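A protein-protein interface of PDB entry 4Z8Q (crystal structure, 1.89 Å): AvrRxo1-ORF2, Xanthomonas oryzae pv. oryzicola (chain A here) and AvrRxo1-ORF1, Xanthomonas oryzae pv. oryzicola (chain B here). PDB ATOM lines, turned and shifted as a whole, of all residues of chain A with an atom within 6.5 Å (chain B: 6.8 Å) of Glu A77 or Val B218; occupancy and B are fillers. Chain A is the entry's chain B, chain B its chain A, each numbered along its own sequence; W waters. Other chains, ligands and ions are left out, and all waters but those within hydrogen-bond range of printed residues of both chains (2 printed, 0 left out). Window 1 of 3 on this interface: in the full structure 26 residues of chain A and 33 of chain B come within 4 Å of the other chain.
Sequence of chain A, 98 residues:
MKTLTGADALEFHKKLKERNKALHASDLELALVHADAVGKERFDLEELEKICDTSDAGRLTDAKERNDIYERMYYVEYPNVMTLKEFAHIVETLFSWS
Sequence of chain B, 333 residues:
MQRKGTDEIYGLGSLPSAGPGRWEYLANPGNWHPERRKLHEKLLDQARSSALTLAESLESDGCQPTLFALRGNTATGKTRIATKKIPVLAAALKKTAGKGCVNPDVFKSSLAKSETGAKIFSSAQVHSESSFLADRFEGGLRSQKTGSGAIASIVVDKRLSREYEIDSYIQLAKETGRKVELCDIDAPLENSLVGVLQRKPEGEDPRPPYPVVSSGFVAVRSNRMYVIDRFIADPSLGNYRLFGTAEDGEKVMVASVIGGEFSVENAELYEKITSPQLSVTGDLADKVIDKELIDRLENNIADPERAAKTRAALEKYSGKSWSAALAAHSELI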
ATOM      1  N   ILE A  69     -16.470  15.489 -22.833  1.00  0.00           N
ATOM      2  CA  ILE A  69     -17.530  15.859 -23.768  1.00  0.00           C
ATOM      3  C   ILE A  69     -18.835  16.153 -23.050  1.00  0.00           C
ATOM      4  O   ILE A  69     -19.445  17.201 -23.252  1.00  0.00           O
ATOM      5  CB  ILE A  69     -17.810  14.750 -24.818  1.00  0.00           C
ATOM      6  CG1 ILE A  69     -16.613  14.547 -25.745  1.00  0.00           C
ATOM      7  CG2 ILE A  69     -19.017  15.099 -25.653  1.00  0.00           C
ATOM      8  CD1 ILE A  69     -15.700  15.718 -25.788  1.00  0.00           C
ATOM      9  N   ARG A  72     -18.765  18.763 -19.799  1.00  0.00           N
ATOM     10  CA  ARG A  72     -18.674  20.116 -20.304  1.00  0.00           C
ATOM     11  C   ARG A  72     -19.940  20.592 -21.039  1.00  0.00           C
ATOM     12  O   ARG A  72     -20.376  21.691 -20.906  1.00  0.00           O
ATOM     13  CB  ARG A  72     -17.431  20.255 -21.157  1.00  0.00           C
ATOM     14  CG  ARG A  72     -17.339  21.553 -21.837  1.00  0.00           C
ATOM     15  CD  ARG A  72     -16.189  21.670 -22.742  1.00  0.00           C
ATOM     16  NE  ARG A  72     -15.034  21.852 -21.933  1.00  0.00           N
ATOM     17  CZ  ARG A  72     -14.592  23.036 -21.533  1.00  0.00           C
ATOM     18  NH1 ARG A  72     -13.570  23.045 -20.778  1.00  0.00           N
ATOM     19  NH2 ARG A  72     -15.149  24.173 -21.923  1.00  0.00           N
ATOM     20  N   MET A  73     -20.530  19.724 -21.811  1.00  0.00           N
ATOM     21  CA  MET A  73     -21.786  20.073 -22.463  1.00  0.00           C
ATOM     22  C   MET A  73     -22.872  20.341 -21.421  1.00  0.00           C
ATOM     23  O   MET A  73     -23.623  21.306 -21.516  1.00  0.00           O
ATOM     24  CB  MET A  73     -22.202  18.941 -23.396  1.00  0.00           C
ATOM     25  CG  MET A  73     -23.483  19.192 -24.127  1.00  0.00           C
ATOM     26  SD  MET A  73     -24.025  17.571 -25.118  1.00  0.00           S
ATOM     27  CE  MET A  73     -22.294  17.241 -25.863  1.00  0.00           C
ATOM     28  N   TYR A  74     -22.930  19.482 -20.407  1.00  0.00           N
ATOM     29  CA  TYR A  74     -23.895  19.602 -19.310  1.00  0.00           C
ATOM     30  C   TYR A  74     -23.806  20.965 -18.607  1.00  0.00           C
ATOM     31  O   TYR A  74     -24.827  21.619 -18.348  1.00  0.00           O
ATOM     32  CB  TYR A  74     -23.658  18.445 -18.314  1.00  0.00           C
ATOM     33  CG  TYR A  74     -24.552  18.412 -17.080  1.00  0.00           C
ATOM     34  CD1 TYR A  74     -25.925  18.226 -17.193  1.00  0.00           C
ATOM     35  CD2 TYR A  74     -24.011  18.549 -15.805  1.00  0.00           C
ATOM     36  CE1 TYR A  74     -26.744  18.193 -16.069  1.00  0.00           C
ATOM     37  CE2 TYR A  74     -24.816  18.511 -14.671  1.00  0.00           C
ATOM     38  CZ  TYR A  74     -26.182  18.332 -14.817  1.00  0.00           C
ATOM     39  OH  TYR A  74     -26.990  18.301 -13.710  1.00  0.00           O
ATOM     40  N   TYR A  75     -22.589  21.399 -18.293  1.00  0.00           N
ATOM     41  CA  TYR A  75     -22.415  22.633 -17.532  1.00  0.00           C
ATOM     42  C   TYR A  75     -22.361  23.878 -18.398  1.00  0.00           C
ATOM     43  O   TYR A  75     -22.928  24.915 -18.044  1.00  0.00           O
ATOM     44  CB  TYR A  75     -21.136  22.575 -16.684  1.00  0.00           C
ATOM     45  CG  TYR A  75     -21.275  21.697 -15.460  1.00  0.00           C
ATOM     46  CD1 TYR A  75     -22.201  22.004 -14.469  1.00  0.00           C
ATOM     47  CD2 TYR A  75     -20.483  20.566 -15.296  1.00  0.00           C
ATOM     48  CE1 TYR A  75     -22.355  21.193 -13.342  1.00  0.00           C
ATOM     49  CE2 TYR A  75     -20.615  19.754 -14.171  1.00  0.00           C
ATOM     50  CZ  TYR A  75     -21.551  20.083 -13.196  1.00  0.00           C
ATOM     51  OH  TYR A  75     -21.687  19.296 -12.079  1.00  0.00           O
ATOM     52  N   VAL A  76     -21.643  23.776 -19.514  1.00  0.00           N
ATOM     53  CA  VAL A  76     -21.328  24.952 -20.304  1.00  0.00           C
ATOM     54  C   VAL A  76     -22.421  25.241 -21.317  1.00  0.00           C
ATOM     55  O   VAL A  76     -22.868  26.376 -21.420  1.00  0.00           O
ATOM     56  CB  VAL A  76     -19.945  24.823 -20.974  1.00  0.00           C
ATOM     57  CG1 VAL A  76     -19.675  25.998 -21.858  1.00  0.00           C
ATOM     58  CG2 VAL A  76     -18.852  24.737 -19.916  1.00  0.00           C
ATOM     59  N   GLU A  77     -22.896  24.208 -22.019  1.00  0.00           N
ATOM     60  CA  GLU A  77     -23.923  24.383 -23.053  1.00  0.00           C
ATOM     61  C   GLU A  77     -25.363  24.332 -22.546  1.00  0.00           C
ATOM     62  O   GLU A  77     -26.265  24.877 -23.184  1.00  0.00           O
ATOM     63  CB  GLU A  77     -23.776  23.326 -24.160  1.00  0.00           C
ATOM     64  CG  GLU A  77     -22.487  23.384 -24.968  1.00  0.00           C
ATOM     65  CD  GLU A  77     -22.508  22.385 -26.109  1.00  0.00           C
ATOM     66  OE1 GLU A  77     -21.569  21.567 -26.231  1.00  0.00           O
ATOM     67  OE2 GLU A  77     -23.486  22.411 -26.886  1.00  0.00           O
ATOM     68  N   TYR A  78     -25.606  23.660 -21.427  1.00  0.00           N
ATOM     69  CA  TYR A  78     -26.983  23.583 -20.927  1.00  0.00           C
ATOM     70  C   TYR A  78     -27.094  23.997 -19.460  1.00  0.00           C
ATOM     71  O   TYR A  78     -27.577  23.219 -18.617  1.00  0.00           O
ATOM     72  CB  TYR A  78     -27.589  22.185 -21.173  1.00  0.00           C
ATOM     73  CG  TYR A  78     -27.648  21.813 -22.650  1.00  0.00           C
ATOM     74  CD1 TYR A  78     -28.704  22.226 -23.453  1.00  0.00           C
ATOM     75  CD2 TYR A  78     -26.634  21.071 -23.237  1.00  0.00           C
ATOM     76  CE1 TYR A  78     -28.752  21.901 -24.817  1.00  0.00           C
ATOM     77  CE2 TYR A  78     -26.674  20.738 -24.591  1.00  0.00           C
ATOM     78  CZ  TYR A  78     -27.733  21.159 -25.371  1.00  0.00           C
ATOM     79  OH  TYR A  78     -27.760  20.836 -26.707  1.00  0.00           O
ATOM     80  N   PRO A  79     -26.683  25.242 -19.157  1.00  0.00           N
ATOM     81  CA  PRO A  79     -26.598  25.696 -17.767  1.00  0.00           C
ATOM     82  C   PRO A  79     -27.958  25.644 -17.076  1.00  0.00           C
ATOM     83  O   PRO A  79     -28.008  25.517 -15.856  1.00  0.00           O
ATOM     84  CB  PRO A  79     -26.138  27.150 -17.906  1.00  0.00           C
ATOM     85  CG  PRO A  79     -26.664  27.584 -19.220  1.00  0.00           C
ATOM     86  CD  PRO A  79     -26.539  26.364 -20.107  1.00  0.00           C
ATOM     87  N   ASN A  80     -29.036  25.731 -17.853  1.00  0.00           N
ATOM     88  CA  ASN A  80     -30.381  25.725 -17.295  1.00  0.00           C
ATOM     89  C   ASN A  80     -30.964  24.331 -17.071  1.00  0.00           C
ATOM     90  O   ASN A  80     -31.991  24.190 -16.408  1.00  0.00           O
ATOM     91  CB  ASN A  80     -31.325  26.563 -18.157  1.00  0.00           C
ATOM     92  CG  ASN A  80     -31.014  28.042 -18.088  1.00  0.00           C
ATOM     93  OD1 ASN A  80     -30.335  28.505 -17.164  1.00  0.00           O
ATOM     94  ND2 ASN A  80     -31.505  28.794 -19.069  1.00  0.00           N
ATOM     95  N   LEU A  94     -29.399  14.031 -29.356  1.00  0.00           N
ATOM     96  CA  LEU A  94     -28.182  14.256 -30.125  1.00  0.00           C
ATOM     97  C   LEU A  94     -27.770  13.017 -30.907  1.00  0.00           C
ATOM     98  O   LEU A  94     -27.303  13.118 -32.041  1.00  0.00           O
ATOM     99  CB  LEU A  94     -27.033  14.736 -29.234  1.00  0.00           C
ATOM    100  CG  LEU A  94     -27.156  16.154 -28.671  1.00  0.00           C
ATOM    101  CD1 LEU A  94     -25.879  16.560 -27.951  1.00  0.00           C
ATOM    102  CD2 LEU A  94     -27.443  17.119 -29.788  1.00  0.00           C
ATOM    103  N   ASN B  73     -20.184  22.059 -39.497  1.00  0.00           N
ATOM    104  CA  ASN B  73     -21.524  21.863 -38.928  1.00  0.00           C
ATOM    105  C   ASN B  73     -22.603  21.757 -40.017  1.00  0.00           C
ATOM    106  O   ASN B  73     -22.357  22.063 -41.179  1.00  0.00           O
ATOM    107  CB  ASN B  73     -21.852  23.015 -37.995  1.00  0.00           C
ATOM    108  CG  ASN B  73     -22.995  22.708 -37.047  1.00  0.00           C
ATOM    109  OD1 ASN B  73     -23.284  21.546 -36.749  1.00  0.00           O
ATOM    110  ND2 ASN B  73     -23.664  23.765 -36.570  1.00  0.00           N
ATOM    111  N   SER B 161     -16.589  16.765 -36.082  1.00  0.00           N
ATOM    112  CA  SER B 161     -16.249  17.802 -35.137  1.00  0.00           C
ATOM    113  C   SER B 161     -15.170  17.312 -34.190  1.00  0.00           C
ATOM    114  O   SER B 161     -14.093  17.924 -34.071  1.00  0.00           O
ATOM    115  CB  SER B 161     -17.484  18.194 -34.368  1.00  0.00           C
ATOM    116  OG  SER B 161     -18.343  18.854 -35.261  1.00  0.00           O
ATOM    117  N   ARG B 162     -15.437  16.163 -33.578  1.00  0.00           N
ATOM    118  CA  ARG B 162     -14.691  15.753 -32.405  1.00  0.00           C
ATOM    119  C   ARG B 162     -13.322  15.181 -32.719  1.00  0.00           C
ATOM    120  O   ARG B 162     -13.093  14.621 -33.785  1.00  0.00           O
ATOM    121  CB  ARG B 162     -15.531  14.795 -31.563  1.00  0.00           C
ATOM    122  CG  ARG B 162     -16.937  15.339 -31.336  1.00  0.00           C
ATOM    123  CD  ARG B 162     -17.364  15.230 -29.880  1.00  0.00           C
ATOM    124  NE  ARG B 162     -18.717  15.747 -29.693  1.00  0.00           N
ATOM    125  CZ  ARG B 162     -19.009  16.923 -29.139  1.00  0.00           C
ATOM    126  NH1 ARG B 162     -20.283  17.309 -29.018  1.00  0.00           N
ATOM    127  NH2 ARG B 162     -18.033  17.710 -28.702  1.00  0.00           N
ATOM    128  N   LEU B 189     -23.835  30.291 -36.392  1.00  0.00           N
ATOM    129  CA  LEU B 189     -24.877  29.360 -35.969  1.00  0.00           C
ATOM    130  C   LEU B 189     -26.216  29.747 -36.593  1.00  0.00           C
ATOM    131  O   LEU B 189     -26.951  28.898 -37.116  1.00  0.00           O
ATOM    132  CB  LEU B 189     -24.967  29.331 -34.423  1.00  0.00           C
ATOM    133  CG  LEU B 189     -26.073  28.454 -33.789  1.00  0.00           C
ATOM    134  CD1 LEU B 189     -25.945  27.024 -34.255  1.00  0.00           C
ATOM    135  CD2 LEU B 189     -26.012  28.469 -32.275  1.00  0.00           C
ATOM    136  N   PRO B 211     -30.927  21.558 -30.666  1.00  0.00           N
ATOM    137  CA  PRO B 211     -29.714  21.176 -29.935  1.00  0.00           C
ATOM    138  C   PRO B 211     -28.675  20.459 -30.790  1.00  0.00           C
ATOM    139  O   PRO B 211     -27.483  20.540 -30.476  1.00  0.00           O
ATOM    140  CB  PRO B 211     -30.248  20.226 -28.859  1.00  0.00           C
ATOM    141  CG  PRO B 211     -31.630  20.718 -28.601  1.00  0.00           C
ATOM    142  CD  PRO B 211     -32.137  21.050 -29.993  1.00  0.00           C
ATOM    143  N   VAL B 213     -27.935  21.199 -33.867  1.00  0.00           N
ATOM    144  CA  VAL B 213     -27.219  22.214 -34.625  1.00  0.00           C
ATOM    145  C   VAL B 213     -26.329  23.046 -33.718  1.00  0.00           C
ATOM    146  O   VAL B 213     -25.181  23.358 -34.063  1.00  0.00           O
ATOM    147  CB  VAL B 213     -28.214  23.124 -35.369  1.00  0.00           C
ATOM    148  CG1 VAL B 213     -27.470  24.127 -36.223  1.00  0.00           C
ATOM    149  CG2 VAL B 213     -29.137  22.265 -36.239  1.00  0.00           C
ATOM    150  N   SER B 214     -26.845  23.407 -32.550  1.00  0.00           N
ATOM    151  CA  SER B 214     -26.045  24.198 -31.603  1.00  0.00           C
ATOM    152  C   SER B 214     -24.857  23.421 -31.018  1.00  0.00           C
ATOM    153  O   SER B 214     -23.717  23.921 -30.971  1.00  0.00           O
ATOM    154  CB  SER B 214     -26.928  24.724 -30.470  1.00  0.00           C
ATOM    155  OG  SER B 214     -26.173  25.542 -29.589  1.00  0.00           O
ATOM    156  N   SER B 215     -25.096  22.198 -30.572  1.00  0.00           N
ATOM    157  CA  SER B 215     -23.983  21.385 -30.052  1.00  0.00           C
ATOM    158  C   SER B 215     -22.987  21.050 -31.155  1.00  0.00           C
ATOM    159  O   SER B 215     -21.776  20.961 -30.907  1.00  0.00           O
ATOM    160  CB  SER B 215     -24.482  20.102 -29.385  1.00  0.00           C
ATOM    161  OG  SER B 215     -25.076  20.417 -28.129  1.00  0.00           O
ATOM    162  N   GLY B 216     -23.483  20.881 -32.379  1.00  0.00           N
ATOM    163  CA  GLY B 216     -22.595  20.661 -33.509  1.00  0.00           C
ATOM    164  C   GLY B 216     -21.707  21.870 -33.753  1.00  0.00           C
ATOM    165  O   GLY B 216     -20.522  21.743 -34.076  1.00  0.00           O
ATOM    166  N   PHE B 217     -22.271  23.057 -33.571  1.00  0.00           N
ATOM    167  CA  PHE B 217     -21.544  24.312 -33.799  1.00  0.00           C
ATOM    168  C   PHE B 217     -20.446  24.496 -32.754  1.00  0.00           C
ATOM    169  O   PHE B 217     -19.280  24.760 -33.083  1.00  0.00           O
ATOM    170  CB  PHE B 217     -22.551  25.460 -33.741  1.00  0.00           C
ATOM    171  CG  PHE B 217     -21.932  26.837 -33.740  1.00  0.00           C
ATOM    172  CD1 PHE B 217     -21.545  27.441 -34.931  1.00  0.00           C
ATOM    173  CD2 PHE B 217     -21.801  27.548 -32.548  1.00  0.00           C
ATOM    174  CE1 PHE B 217     -21.004  28.721 -34.931  1.00  0.00           C
ATOM    175  CE2 PHE B 217     -21.271  28.840 -32.538  1.00  0.00           C
ATOM    176  CZ  PHE B 217     -20.872  29.421 -33.727  1.00  0.00           C
ATOM    177  N   VAL B 218     -20.813  24.328 -31.494  1.00  0.00           N
ATOM    178  CA  VAL B 218     -19.835  24.361 -30.411  1.00  0.00           C
ATOM    179  C   VAL B 218     -18.689  23.384 -30.633  1.00  0.00           C
ATOM    180  O   VAL B 218     -17.514  23.738 -30.475  1.00  0.00           O
ATOM    181  CB  VAL B 218     -20.501  24.088 -29.053  1.00  0.00           C
ATOM    182  CG1 VAL B 218     -19.440  23.938 -27.951  1.00  0.00           C
ATOM    183  CG2 VAL B 218     -21.468  25.230 -28.714  1.00  0.00           C
ATOM    184  N   ALA B 219     -19.014  22.149 -30.996  1.00  0.00           N
ATOM    185  CA  ALA B 219     -17.990  21.126 -31.150  1.00  0.00           C
ATOM    186  C   ALA B 219     -17.079  21.427 -32.338  1.00  0.00           C
ATOM    187  O   ALA B 219     -15.861  21.248 -32.274  1.00  0.00           O
ATOM    188  CB  ALA B 219     -18.642  19.739 -31.302  1.00  0.00           C
ATOM    189  N   VAL B 220     -17.661  21.883 -33.438  1.00  0.00           N
ATOM    190  CA  VAL B 220     -16.846  22.121 -34.624  1.00  0.00           C
ATOM    191  C   VAL B 220     -15.859  23.273 -34.395  1.00  0.00           C
ATOM    192  O   VAL B 220     -14.710  23.211 -34.826  1.00  0.00           O
ATOM    193  CB  VAL B 220     -17.740  22.317 -35.885  1.00  0.00           C
ATOM    194  CG1 VAL B 220     -18.193  23.740 -36.028  1.00  0.00           C
ATOM    195  CG2 VAL B 220     -17.024  21.867 -37.140  1.00  0.00           C
ATOM    196  N   ARG B 221     -16.299  24.298 -33.677  1.00  0.00           N
ATOM    197  CA  ARG B 221     -15.464  25.451 -33.401  1.00  0.00           C
ATOM    198  C   ARG B 221     -14.359  25.113 -32.390  1.00  0.00           C
ATOM    199  O   ARG B 221     -13.193  25.417 -32.622  1.00  0.00           O
ATOM    200  CB  ARG B 221     -16.331  26.596 -32.878  1.00  0.00           C
ATOM    201  CG  ARG B 221     -17.218  27.257 -33.965  1.00  0.00           C
ATOM    202  CD  ARG B 221     -16.736  28.645 -34.301  1.00  0.00           C
ATOM    203  NE  ARG B 221     -17.455  29.308 -35.404  1.00  0.00           N
ATOM    204  CZ  ARG B 221     -18.035  30.503 -35.291  1.00  0.00           C
ATOM    205  NH1 ARG B 221     -18.010  31.139 -34.126  1.00  0.00           N
ATOM    206  NH2 ARG B 221     -18.656  31.061 -36.328  1.00  0.00           N
ATOM    207  N   SER B 222     -14.749  24.496 -31.276  1.00  0.00           N
ATOM    208  CA  SER B 222     -13.826  24.191 -30.190  1.00  0.00           C
ATOM    209  C   SER B 222     -12.684  23.285 -30.605  1.00  0.00           C
ATOM    210  O   SER B 222     -11.568  23.400 -30.084  1.00  0.00           O
ATOM    211  CB  SER B 222     -14.587  23.566 -29.016  1.00  0.00           C
ATOM    212  OG  SER B 222     -15.403  24.559 -28.416  1.00  0.00           O
ATOM    213  N   ASN B 223     -12.952  22.396 -31.554  1.00  0.00           N
ATOM    214  CA  ASN B 223     -11.974  21.383 -31.932  1.00  0.00           C
ATOM    215  C   ASN B 223     -11.304  21.667 -33.263  1.00  0.00           C
ATOM    216  O   ASN B 223     -10.545  20.860 -33.756  1.00  0.00           O
ATOM    217  CB  ASN B 223     -12.623  20.001 -31.946  1.00  0.00           C
ATOM    218  CG  ASN B 223     -13.073  19.578 -30.579  1.00  0.00           C
ATOM    219  OD1 ASN B 223     -12.283  19.585 -29.630  1.00  0.00           O
ATOM    220  ND2 ASN B 223     -14.346  19.238 -30.449  1.00  0.00           N
ATOM    221  N   SER B 275     -13.713  29.718 -31.884  1.00  0.00           N
ATOM    222  CA  SER B 275     -14.342  29.623 -30.568  1.00  0.00           C
ATOM    223  C   SER B 275     -15.861  29.693 -30.649  1.00  0.00           C
ATOM    224  O   SER B 275     -16.404  30.321 -31.556  1.00  0.00           O
ATOM    225  CB  SER B 275     -13.779  30.686 -29.620  1.00  0.00           C
ATOM    226  OG  SER B 275     -14.392  31.938 -29.827  1.00  0.00           O
ATOM    227  N   PRO B 276     -16.562  29.059 -29.689  1.00  0.00           N
ATOM    228  CA  PRO B 276     -18.018  28.929 -29.837  1.00  0.00           C
ATOM    229  C   PRO B 276     -18.822  30.192 -29.512  1.00  0.00           C
ATOM    230  O   PRO B 276     -20.050  30.162 -29.651  1.00  0.00           O
ATOM    231  CB  PRO B 276     -18.385  27.811 -28.847  1.00  0.00           C
ATOM    232  CG  PRO B 276     -17.077  27.340 -28.227  1.00  0.00           C
ATOM    233  CD  PRO B 276     -16.081  28.437 -28.444  1.00  0.00           C
ATOM    234  N   LEU B 278     -19.989  31.747 -26.788  1.00  0.00           N
ATOM    235  CA  LEU B 278     -21.158  31.271 -26.033  1.00  0.00           C
ATOM    236  C   LEU B 278     -22.237  32.314 -25.701  1.00  0.00           C
ATOM    237  O   LEU B 278     -23.258  31.987 -25.087  1.00  0.00           O
ATOM    238  CB  LEU B 278     -20.720  30.555 -24.759  1.00  0.00           C
ATOM    239  CG  LEU B 278     -19.759  29.393 -24.986  1.00  0.00           C
ATOM    240  CD1 LEU B 278     -19.382  28.833 -23.653  1.00  0.00           C
ATOM    241  CD2 LEU B 278     -20.382  28.316 -25.859  1.00  0.00           C
ATOM    242  N   ASP B 283     -29.118  33.168 -24.728  1.00  0.00           N
ATOM    243  CA  ASP B 283     -28.676  32.388 -25.879  1.00  0.00           C
ATOM    244  C   ASP B 283     -29.727  32.345 -26.991  1.00  0.00           C
ATOM    245  O   ASP B 283     -30.843  32.849 -26.845  1.00  0.00           O
ATOM    246  CB  ASP B 283     -28.334  30.959 -25.466  1.00  0.00           C
ATOM    247  CG  ASP B 283     -29.553  30.057 -25.460  1.00  0.00           C
ATOM    248  OD1 ASP B 283     -30.460  30.286 -24.623  1.00  0.00           O
ATOM    249  OD2 ASP B 283     -29.607  29.126 -26.298  1.00  0.00           O
HETATM  250  O   HOH W   1     -21.148  20.300 -28.322  1.00  0.00           O
HETATM  251  O   HOH W   2     -25.214  24.449 -27.474  1.00  0.00           O
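Among the printed residues, merely in contact across the chains: Ile A69 with Arg B162 (3.9 Å), Met A73 with Arg B162 (3.7 Å), Val A76 with Leu B278 (3.4 Å), Glu A77 with Val B218 (3.6 Å), Tyr A78 with Pro B211 (3.3 Å), Leu A94 with Pro B211 (3.5 Å) and Leu A94 with Ser B215 (3.9 Å).
Glu A77 touches just these residues of chain B: Ser B215 and Val B218.
Of chain A, only Glu A77 (3.6 Å) comes within 4 Å of Val B218.
Of the printed residues of chain B, Met A73 touches Arg B162 (3.7 Å).
Of the printed residues of chain A, Arg B162 touches Ile A69 (3.9 Å) and Met A73 (3.7 Å).
Of the printed residues of chain B, Ile A69 touches Arg B162.
Printed residues of chain A within 4 Å of Pro B211: Tyr A78 (3.3 Å) and Leu A94 (3.5 Å).
Printed residues of chain B within 4 Å of Val A76: Leu B278.
Asn B223 touches none of the printed residues of chain A.
OG of Ser B215 is in hydrogen-bond range of OE2 of Glu A77 (2.8 Å).
The side-chain hydroxyl (OG) of Ser B215 lies within hydrogen-bond range of the side-chain hydroxyl (OH) of Tyr A78.
Water W1 lies within hydrogen-bond range of the side-chain carboxylate (OE1) of Glu A77 (2.5 Å), the backbone carbonyl oxygen (O) of Ser B215 (2.7 Å) and the guanidinium group (NH1) of Arg B162 (3.2 Å).
Water W2 bridges OG of Ser B214 (2.6 Å) and OE2 of Glu A77 (2.7 Å).
The backbone carbonyl oxygen of Met A73 lies within hydrogen-bond range of the backbone NH of Tyr A78, 3.1 Å away.
The backbone carbonyl oxygen (O) of Pro B211 sits close to the side-chain hydroxyl (OG) of Ser B215.
The backbone carbonyl oxygen of Val B218 is in hydrogen-bond range of the side-chain hydroxyl of Ser B222 (3.1 Å).
Of the 20 printed residues of chain B, 5 touch a printed residue of chain A.
Of the 11 printed residues of chain A, 6 touch a printed residue of chain B.
Hydrophobic or aromatic side chains of chain A within 4 Å of the printed part of chain B: Ile A69, Met A73, Val A76, Tyr A78 and Leu A94.
Along chain A the printed residues that touch a printed residue of chain B span positions 69 to 94.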
